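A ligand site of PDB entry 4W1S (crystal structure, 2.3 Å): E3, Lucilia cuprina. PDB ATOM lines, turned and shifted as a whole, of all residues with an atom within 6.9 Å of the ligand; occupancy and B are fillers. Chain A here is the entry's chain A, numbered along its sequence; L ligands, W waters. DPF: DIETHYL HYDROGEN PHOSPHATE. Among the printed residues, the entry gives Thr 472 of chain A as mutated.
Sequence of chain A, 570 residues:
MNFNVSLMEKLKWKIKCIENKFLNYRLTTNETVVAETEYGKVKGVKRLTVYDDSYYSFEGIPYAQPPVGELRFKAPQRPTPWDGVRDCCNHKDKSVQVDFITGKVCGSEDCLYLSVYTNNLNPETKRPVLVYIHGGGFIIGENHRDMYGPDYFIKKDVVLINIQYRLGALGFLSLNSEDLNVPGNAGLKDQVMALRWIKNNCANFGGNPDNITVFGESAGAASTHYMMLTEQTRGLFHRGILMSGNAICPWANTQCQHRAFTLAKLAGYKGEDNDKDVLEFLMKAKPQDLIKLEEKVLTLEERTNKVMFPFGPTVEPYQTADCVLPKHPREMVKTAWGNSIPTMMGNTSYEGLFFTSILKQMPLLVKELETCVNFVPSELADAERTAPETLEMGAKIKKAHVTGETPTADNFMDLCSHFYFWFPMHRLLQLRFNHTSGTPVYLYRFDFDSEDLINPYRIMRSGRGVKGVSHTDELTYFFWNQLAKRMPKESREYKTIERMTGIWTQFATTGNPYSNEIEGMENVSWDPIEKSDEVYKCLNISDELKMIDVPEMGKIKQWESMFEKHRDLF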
ATOM      1  N   HIS A 134      11.082 -20.218 -12.352  1.00  0.00           N
ATOM      2  CA  HIS A 134      11.876 -19.424 -11.406  1.00  0.00           C
ATOM      3  C   HIS A 134      11.937 -20.073 -10.022  1.00  0.00           C
ATOM      4  O   HIS A 134      11.053 -20.815  -9.634  1.00  0.00           O
ATOM      5  CB  HIS A 134      11.327 -18.011 -11.296  1.00  0.00           C
ATOM      6  CG  HIS A 134      10.043 -17.905 -10.524  1.00  0.00           C
ATOM      7  ND1 HIS A 134       9.997 -17.898  -9.148  1.00  0.00           N
ATOM      8  CD2 HIS A 134       8.763 -17.770 -10.950  1.00  0.00           C
ATOM      9  CE1 HIS A 134       8.745 -17.767  -8.753  1.00  0.00           C
ATOM     10  NE2 HIS A 134       7.986 -17.676  -9.821  1.00  0.00           N
ATOM     11  N   GLY A 135      13.022 -19.803  -9.292  1.00  0.00           N
ATOM     12  CA  GLY A 135      13.155 -20.249  -7.932  1.00  0.00           C
ATOM     13  C   GLY A 135      12.679 -19.168  -6.999  1.00  0.00           C
ATOM     14  O   GLY A 135      12.006 -18.222  -7.431  1.00  0.00           O
ATOM     15  N   GLY A 136      13.043 -19.266  -5.721  1.00  0.00           N
ATOM     16  CA  GLY A 136      12.491 -18.389  -4.702  1.00  0.00           C
ATOM     17  C   GLY A 136      11.843 -19.185  -3.589  1.00  0.00           C
ATOM     18  O   GLY A 136      10.899 -18.715  -2.936  1.00  0.00           O
ATOM     19  N   GLY A 137      12.368 -20.396  -3.385  1.00  0.00           N
ATOM     20  CA  GLY A 137      11.962 -21.257  -2.283  1.00  0.00           C
ATOM     21  C   GLY A 137      10.472 -21.481  -2.178  1.00  0.00           C
ATOM     22  O   GLY A 137       9.972 -21.773  -1.105  1.00  0.00           O
ATOM     23  N   PHE A 138       9.779 -21.337  -3.304  1.00  0.00           N
ATOM     24  CA  PHE A 138       8.324 -21.528  -3.405  1.00  0.00           C
ATOM     25  C   PHE A 138       7.517 -20.449  -2.694  1.00  0.00           C
ATOM     26  O   PHE A 138       6.284 -20.560  -2.569  1.00  0.00           O
ATOM     27  CB  PHE A 138       7.910 -22.903  -2.863  1.00  0.00           C
ATOM     28  CG  PHE A 138       8.441 -24.053  -3.669  1.00  0.00           C
ATOM     29  CD1 PHE A 138       8.036 -24.223  -4.987  1.00  0.00           C
ATOM     30  CD2 PHE A 138       9.324 -24.970  -3.113  1.00  0.00           C
ATOM     31  CE1 PHE A 138       8.513 -25.300  -5.741  1.00  0.00           C
ATOM     32  CE2 PHE A 138       9.798 -26.041  -3.851  1.00  0.00           C
ATOM     33  CZ  PHE A 138       9.381 -26.205  -5.180  1.00  0.00           C
ATOM     34  N   ILE A 140       8.817 -16.688  -2.945  1.00  0.00           N
ATOM     35  CA  ILE A 140       8.985 -15.437  -3.713  1.00  0.00           C
ATOM     36  C   ILE A 140       9.286 -15.729  -5.180  1.00  0.00           C
ATOM     37  O   ILE A 140       9.576 -16.876  -5.529  1.00  0.00           O
ATOM     38  CB  ILE A 140      10.141 -14.528  -3.171  1.00  0.00           C
ATOM     39  CG1 ILE A 140      11.495 -15.236  -3.277  1.00  0.00           C
ATOM     40  CG2 ILE A 140       9.847 -14.039  -1.738  1.00  0.00           C
ATOM     41  CD1 ILE A 140      12.657 -14.310  -3.350  1.00  0.00           C
ATOM     42  N   GLU A 217      16.121 -23.002 -11.540  1.00  0.00           N
ATOM     43  CA  GLU A 217      17.185 -22.842 -10.567  1.00  0.00           C
ATOM     44  C   GLU A 217      16.585 -22.782  -9.141  1.00  0.00           C
ATOM     45  O   GLU A 217      15.546 -22.191  -8.952  1.00  0.00           O
ATOM     46  CB  GLU A 217      17.988 -21.591 -10.924  1.00  0.00           C
ATOM     47  CG  GLU A 217      19.302 -21.436 -10.193  1.00  0.00           C
ATOM     48  CD  GLU A 217      19.191 -20.478  -9.030  1.00  0.00           C
ATOM     49  OE1 GLU A 217      18.351 -19.546  -9.099  1.00  0.00           O
ATOM     50  OE2 GLU A 217      19.936 -20.677  -8.043  1.00  0.00           O
ATOM     51  N   SER A 218      17.224 -23.448  -8.165  1.00  0.00           N
ATOM     52  CA  SER A 218      16.788 -23.435  -6.744  1.00  0.00           C
ATOM     53  C   SER A 218      15.460 -24.211  -6.542  1.00  0.00           C
ATOM     54  O   SER A 218      15.374 -25.418  -6.803  1.00  0.00           O
ATOM     55  CB  SER A 218      16.658 -21.988  -6.252  1.00  0.00           C
ATOM     56  OG  SER A 218      16.591 -21.881  -4.835  1.00  0.00           O
ATOM     57  N   ALA A 219      14.420 -23.512  -6.088  1.00  0.00           N
ATOM     58  CA  ALA A 219      13.059 -24.058  -6.069  1.00  0.00           C
ATOM     59  C   ALA A 219      12.570 -24.280  -7.494  1.00  0.00           C
ATOM     60  O   ALA A 219      11.678 -25.096  -7.727  1.00  0.00           O
ATOM     61  CB  ALA A 219      12.108 -23.119  -5.344  1.00  0.00           C
ATOM     62  N   GLY A 220      13.118 -23.512  -8.439  1.00  0.00           N
ATOM     63  CA  GLY A 220      12.880 -23.718  -9.853  1.00  0.00           C
ATOM     64  C   GLY A 220      13.489 -25.027 -10.339  1.00  0.00           C
ATOM     65  O   GLY A 220      12.936 -25.701 -11.214  1.00  0.00           O
ATOM     66  N   ALA A 221      14.613 -25.401  -9.735  1.00  0.00           N
ATOM     67  CA  ALA A 221      15.237 -26.667 -10.060  1.00  0.00           C
ATOM     68  C   ALA A 221      14.417 -27.832  -9.507  1.00  0.00           C
ATOM     69  O   ALA A 221      14.238 -28.820 -10.199  1.00  0.00           O
ATOM     70  CB  ALA A 221      16.663 -26.721  -9.539  1.00  0.00           C
ATOM     71  N   SER A 244      21.321 -26.256  -9.454  1.00  0.00           N
ATOM     72  CA  SER A 244      21.368 -26.135  -7.986  1.00  0.00           C
ATOM     73  C   SER A 244      20.079 -26.595  -7.308  1.00  0.00           C
ATOM     74  O   SER A 244      19.486 -25.852  -6.533  1.00  0.00           O
ATOM     75  CB  SER A 244      21.648 -24.684  -7.551  1.00  0.00           C
ATOM     76  OG  SER A 244      22.881 -24.205  -8.053  1.00  0.00           O
ATOM     77  N   TRP A 251      14.950 -29.133   1.606  1.00  0.00           N
ATOM     78  CA  TRP A 251      14.007 -28.009   1.587  1.00  0.00           C
ATOM     79  C   TRP A 251      12.861 -28.144   0.560  1.00  0.00           C
ATOM     80  O   TRP A 251      11.949 -27.322   0.557  1.00  0.00           O
ATOM     81  CB  TRP A 251      14.764 -26.696   1.300  1.00  0.00           C
ATOM     82  CG  TRP A 251      15.731 -26.845   0.179  1.00  0.00           C
ATOM     83  CD1 TRP A 251      17.057 -27.172   0.291  1.00  0.00           C
ATOM     84  CD2 TRP A 251      15.466 -26.724  -1.221  1.00  0.00           C
ATOM     85  NE1 TRP A 251      17.634 -27.243  -0.948  1.00  0.00           N
ATOM     86  CE2 TRP A 251      16.685 -26.977  -1.900  1.00  0.00           C
ATOM     87  CE3 TRP A 251      14.328 -26.429  -1.973  1.00  0.00           C
ATOM     88  CZ2 TRP A 251      16.781 -26.948  -3.300  1.00  0.00           C
ATOM     89  CZ3 TRP A 251      14.421 -26.393  -3.357  1.00  0.00           C
ATOM     90  CH2 TRP A 251      15.650 -26.647  -4.010  1.00  0.00           C
ATOM     91  N   ALA A 252      12.897 -29.180  -0.289  1.00  0.00           N
ATOM     92  CA  ALA A 252      12.009 -29.241  -1.460  1.00  0.00           C
ATOM     93  C   ALA A 252      10.688 -29.983  -1.245  1.00  0.00           C
ATOM     94  O   ALA A 252       9.855 -30.062  -2.152  1.00  0.00           O
ATOM     95  CB  ALA A 252      12.734 -29.863  -2.642  1.00  0.00           C
ATOM     96  N   MET A 308      12.910 -25.235   6.434  1.00  0.00           N
ATOM     97  CA  MET A 308      13.221 -23.899   5.964  1.00  0.00           C
ATOM     98  C   MET A 308      11.962 -23.055   5.751  1.00  0.00           C
ATOM     99  O   MET A 308      11.917 -21.868   6.115  1.00  0.00           O
ATOM    100  CB  MET A 308      14.032 -23.976   4.667  1.00  0.00           C
ATOM    101  CG  MET A 308      14.907 -22.748   4.449  1.00  0.00           C
ATOM    102  SD  MET A 308      15.766 -22.745   2.870  1.00  0.00           S
ATOM    103  CE  MET A 308      17.032 -23.961   3.194  1.00  0.00           C
ATOM    104  N   PHE A 309      10.934 -23.690   5.174  1.00  0.00           N
ATOM    105  CA  PHE A 309       9.684 -23.025   4.847  1.00  0.00           C
ATOM    106  C   PHE A 309       8.491 -23.809   5.392  1.00  0.00           C
ATOM    107  O   PHE A 309       8.495 -25.031   5.369  1.00  0.00           O
ATOM    108  CB  PHE A 309       9.546 -22.867   3.330  1.00  0.00           C
ATOM    109  CG  PHE A 309      10.781 -22.357   2.650  1.00  0.00           C
ATOM    110  CD1 PHE A 309      11.098 -21.014   2.664  1.00  0.00           C
ATOM    111  CD2 PHE A 309      11.620 -23.235   1.966  1.00  0.00           C
ATOM    112  CE1 PHE A 309      12.229 -20.531   2.026  1.00  0.00           C
ATOM    113  CE2 PHE A 309      12.760 -22.753   1.317  1.00  0.00           C
ATOM    114  CZ  PHE A 309      13.053 -21.386   1.355  1.00  0.00           C
ATOM    115  N   PHE A 354      25.997 -18.294   0.020  1.00  0.00           N
ATOM    116  CA  PHE A 354      24.738 -17.598   0.115  1.00  0.00           C
ATOM    117  C   PHE A 354      24.386 -17.209   1.550  1.00  0.00           C
ATOM    118  O   PHE A 354      23.892 -16.115   1.810  1.00  0.00           O
ATOM    119  CB  PHE A 354      23.639 -18.493  -0.490  1.00  0.00           C
ATOM    120  CG  PHE A 354      22.281 -17.864  -0.505  1.00  0.00           C
ATOM    121  CD1 PHE A 354      21.445 -17.951   0.592  1.00  0.00           C
ATOM    122  CD2 PHE A 354      21.846 -17.172  -1.626  1.00  0.00           C
ATOM    123  CE1 PHE A 354      20.194 -17.370   0.569  1.00  0.00           C
ATOM    124  CE2 PHE A 354      20.597 -16.586  -1.657  1.00  0.00           C
ATOM    125  CZ  PHE A 354      19.766 -16.684  -0.554  1.00  0.00           C
ATOM    126  N   PHE A 355      24.646 -18.118   2.483  1.00  0.00           N
ATOM    127  CA  PHE A 355      24.155 -17.990   3.859  1.00  0.00           C
ATOM    128  C   PHE A 355      24.918 -17.025   4.732  1.00  0.00           C
ATOM    129  O   PHE A 355      24.683 -17.008   5.942  1.00  0.00           O
ATOM    130  CB  PHE A 355      24.182 -19.348   4.550  1.00  0.00           C
ATOM    131  CG  PHE A 355      23.172 -20.315   4.016  1.00  0.00           C
ATOM    132  CD1 PHE A 355      21.911 -20.411   4.585  1.00  0.00           C
ATOM    133  CD2 PHE A 355      23.479 -21.132   2.940  1.00  0.00           C
ATOM    134  CE1 PHE A 355      20.978 -21.291   4.095  1.00  0.00           C
ATOM    135  CE2 PHE A 355      22.533 -22.023   2.439  1.00  0.00           C
ATOM    136  CZ  PHE A 355      21.285 -22.108   3.019  1.00  0.00           C
ATOM    137  N   TYR A 420      22.427 -28.857   1.612  1.00  0.00           N
ATOM    138  CA  TYR A 420      21.343 -28.408   0.757  1.00  0.00           C
ATOM    139  C   TYR A 420      21.455 -28.766  -0.730  1.00  0.00           C
ATOM    140  O   TYR A 420      20.428 -28.804  -1.405  1.00  0.00           O
ATOM    141  CB  TYR A 420      21.182 -26.891   0.888  1.00  0.00           C
ATOM    142  CG  TYR A 420      20.729 -26.477   2.254  1.00  0.00           C
ATOM    143  CD1 TYR A 420      19.452 -26.796   2.708  1.00  0.00           C
ATOM    144  CD2 TYR A 420      21.573 -25.755   3.097  1.00  0.00           C
ATOM    145  CE1 TYR A 420      19.023 -26.423   3.975  1.00  0.00           C
ATOM    146  CE2 TYR A 420      21.144 -25.371   4.372  1.00  0.00           C
ATOM    147  CZ  TYR A 420      19.870 -25.708   4.802  1.00  0.00           C
ATOM    148  OH  TYR A 420      19.436 -25.334   6.055  1.00  0.00           O
ATOM    149  N   PHE A 421      22.663 -29.037  -1.249  1.00  0.00           N
ATOM    150  CA  PHE A 421      22.814 -29.272  -2.699  1.00  0.00           C
ATOM    151  C   PHE A 421      23.647 -30.494  -3.154  1.00  0.00           C
ATOM    152  O   PHE A 421      23.144 -31.323  -3.902  1.00  0.00           O
ATOM    153  CB  PHE A 421      23.374 -28.011  -3.362  1.00  0.00           C
ATOM    154  CG  PHE A 421      22.560 -26.759  -3.069  1.00  0.00           C
ATOM    155  CD1 PHE A 421      21.364 -26.536  -3.737  1.00  0.00           C
ATOM    156  CD2 PHE A 421      22.997 -25.835  -2.132  1.00  0.00           C
ATOM    157  CE1 PHE A 421      20.610 -25.399  -3.462  1.00  0.00           C
ATOM    158  CE2 PHE A 421      22.243 -24.698  -1.856  1.00  0.00           C
ATOM    159  CZ  PHE A 421      21.052 -24.486  -2.519  1.00  0.00           C
ATOM    160  N   TYR A 457      19.609 -10.972  -6.166  1.00  0.00           N
ATOM    161  CA  TYR A 457      19.867 -11.860  -5.030  1.00  0.00           C
ATOM    162  C   TYR A 457      21.163 -11.525  -4.287  1.00  0.00           C
ATOM    163  O   TYR A 457      21.328 -11.907  -3.138  1.00  0.00           O
ATOM    164  CB  TYR A 457      19.923 -13.313  -5.482  1.00  0.00           C
ATOM    165  CG  TYR A 457      18.573 -13.880  -5.826  1.00  0.00           C
ATOM    166  CD1 TYR A 457      17.760 -14.430  -4.843  1.00  0.00           C
ATOM    167  CD2 TYR A 457      18.101 -13.878  -7.138  1.00  0.00           C
ATOM    168  CE1 TYR A 457      16.521 -14.954  -5.141  1.00  0.00           C
ATOM    169  CE2 TYR A 457      16.863 -14.395  -7.444  1.00  0.00           C
ATOM    170  CZ  TYR A 457      16.077 -14.936  -6.447  1.00  0.00           C
ATOM    171  OH  TYR A 457      14.840 -15.466  -6.761  1.00  0.00           O
ATOM    172  N   MET A 460      20.102  -9.464  -1.414  1.00  0.00           N
ATOM    173  CA  MET A 460      19.490 -10.279  -0.382  1.00  0.00           C
ATOM    174  C   MET A 460      20.517 -10.984   0.513  1.00  0.00           C
ATOM    175  O   MET A 460      20.519 -10.788   1.723  1.00  0.00           O
ATOM    176  CB  MET A 460      18.569 -11.315  -1.031  1.00  0.00           C
ATOM    177  CG  MET A 460      17.851 -12.214  -0.048  1.00  0.00           C
ATOM    178  SD  MET A 460      17.033 -13.592  -0.879  1.00  0.00           S
ATOM    179  CE  MET A 460      15.829 -12.727  -1.880  1.00  0.00           C
ATOM    180  N   HIS A 471      25.367 -19.572  -4.715  1.00  0.00           N
ATOM    181  CA  HIS A 471      24.064 -19.938  -5.255  1.00  0.00           C
ATOM    182  C   HIS A 471      23.388 -18.688  -5.847  1.00  0.00           C
ATOM    183  O   HIS A 471      23.401 -17.619  -5.200  1.00  0.00           O
ATOM    184  CB  HIS A 471      23.210 -20.591  -4.142  1.00  0.00           C
ATOM    185  CG  HIS A 471      21.858 -21.058  -4.578  1.00  0.00           C
ATOM    186  ND1 HIS A 471      20.706 -20.396  -4.229  1.00  0.00           N
ATOM    187  CD2 HIS A 471      21.477 -22.134  -5.309  1.00  0.00           C
ATOM    188  CE1 HIS A 471      19.665 -21.031  -4.733  1.00  0.00           C
ATOM    189  NE2 HIS A 471      20.103 -22.082  -5.391  1.00  0.00           N
ATOM    190  N   THR A 472      22.824 -18.837  -7.050  1.00  0.00           N
ATOM    191  CA  THR A 472      22.178 -17.773  -7.868  1.00  0.00           C
ATOM    192  C   THR A 472      23.122 -16.806  -8.583  1.00  0.00           C
ATOM    193  O   THR A 472      22.653 -15.982  -9.365  1.00  0.00           O
ATOM    194  CB  THR A 472      21.186 -16.855  -7.093  1.00  0.00           C
ATOM    195  OG1 THR A 472      21.925 -15.893  -6.317  1.00  0.00           O
ATOM    196  CG2 THR A 472      20.244 -17.667  -6.217  1.00  0.00           C
ATOM    197  N   LEU A 475      22.748 -16.850 -12.441  1.00  0.00           N
ATOM    198  CA  LEU A 475      21.581 -16.287 -13.122  1.00  0.00           C
ATOM    199  C   LEU A 475      21.947 -15.022 -13.867  1.00  0.00           C
ATOM    200  O   LEU A 475      21.300 -14.639 -14.836  1.00  0.00           O
ATOM    201  CB  LEU A 475      20.463 -15.987 -12.131  1.00  0.00           C
ATOM    202  CG  LEU A 475      19.727 -17.199 -11.579  1.00  0.00           C
ATOM    203  CD1 LEU A 475      18.698 -16.726 -10.568  1.00  0.00           C
ATOM    204  CD2 LEU A 475      19.085 -18.019 -12.719  1.00  0.00           C
HETATM  205  O4  DPF L   1      14.805 -21.188  -4.485  1.00  0.00           O
HETATM  206  P1  DPF L   1      16.138 -20.913  -3.839  1.00  0.00           P
HETATM  207  O3  DPF L   1      16.022 -21.527  -2.273  1.00  0.00           O
HETATM  208  C1  DPF L   1      15.880 -22.896  -2.124  1.00  0.00           C
HETATM  209  C4  DPF L   1      16.450 -23.311  -0.771  1.00  0.00           C
HETATM  210  O1  DPF L   1      16.121 -19.282  -3.551  1.00  0.00           O
HETATM  211  C2  DPF L   1      16.861 -18.466  -4.387  1.00  0.00           C
HETATM  212  C3  DPF L   1      18.027 -17.867  -3.613  1.00  0.00           C
HETATM  213  O   HOH W   1      16.487 -19.131  -7.573  1.00  0.00           O
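The side-chain hydroxyl (OG) of Ser 218 is bonded to a phosphorus (P1) of the ligand.
N of Gly 137 is in hydrogen-bond range of O4 of the ligand, at 2.8 Å.
The backbone NH (N) of Ala 219 is in hydrogen-bond range of an oxygen (O4) of the ligand, 2.8 Å away.
The backbone NH of Gly 136 sits at hydrogen-bond distance from an oxygen (O4) of the ligand, 2.9 Å away.
The indole nitrogen of Trp 251 lies within hydrogen-bond range of the backbone carbonyl oxygen of Tyr 420, 3.2 Å away.
The side-chain carboxylate (OE2) of Glu 217 sits at hydrogen-bond distance from a ring nitrogen (NE2) of His 471, 3.0 Å away.
N of Gly 135 lies close to O of Glu 217, at 3.5 Å.
Gly 135 touches the ligand (C to O4, 3.9 Å).
Trp 251 touches the ligand (CD2 to C4, 3.6 Å).
Met 308 touches the ligand (SD to C4, 3.7 Å).
CE2 of Phe 354 touches C3 of the ligand (3.5 Å).
Tyr 457 touches the ligand.
His 471 touches the ligand (CE1 to P1, 3.6 Å).
CG2 of Thr 472 touches C3 of the ligand (3.4 Å).
11 residues have an atom within 4 Å of the ligand: Gly 135, Gly 136, Gly 137, Ser 218, Ala 219, Trp 251, Met 308, Phe 354, Tyr 457, His 471 and Thr 472.
The nearest printed residue that does not touch the ligand is Phe 309 (4.3 Å).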
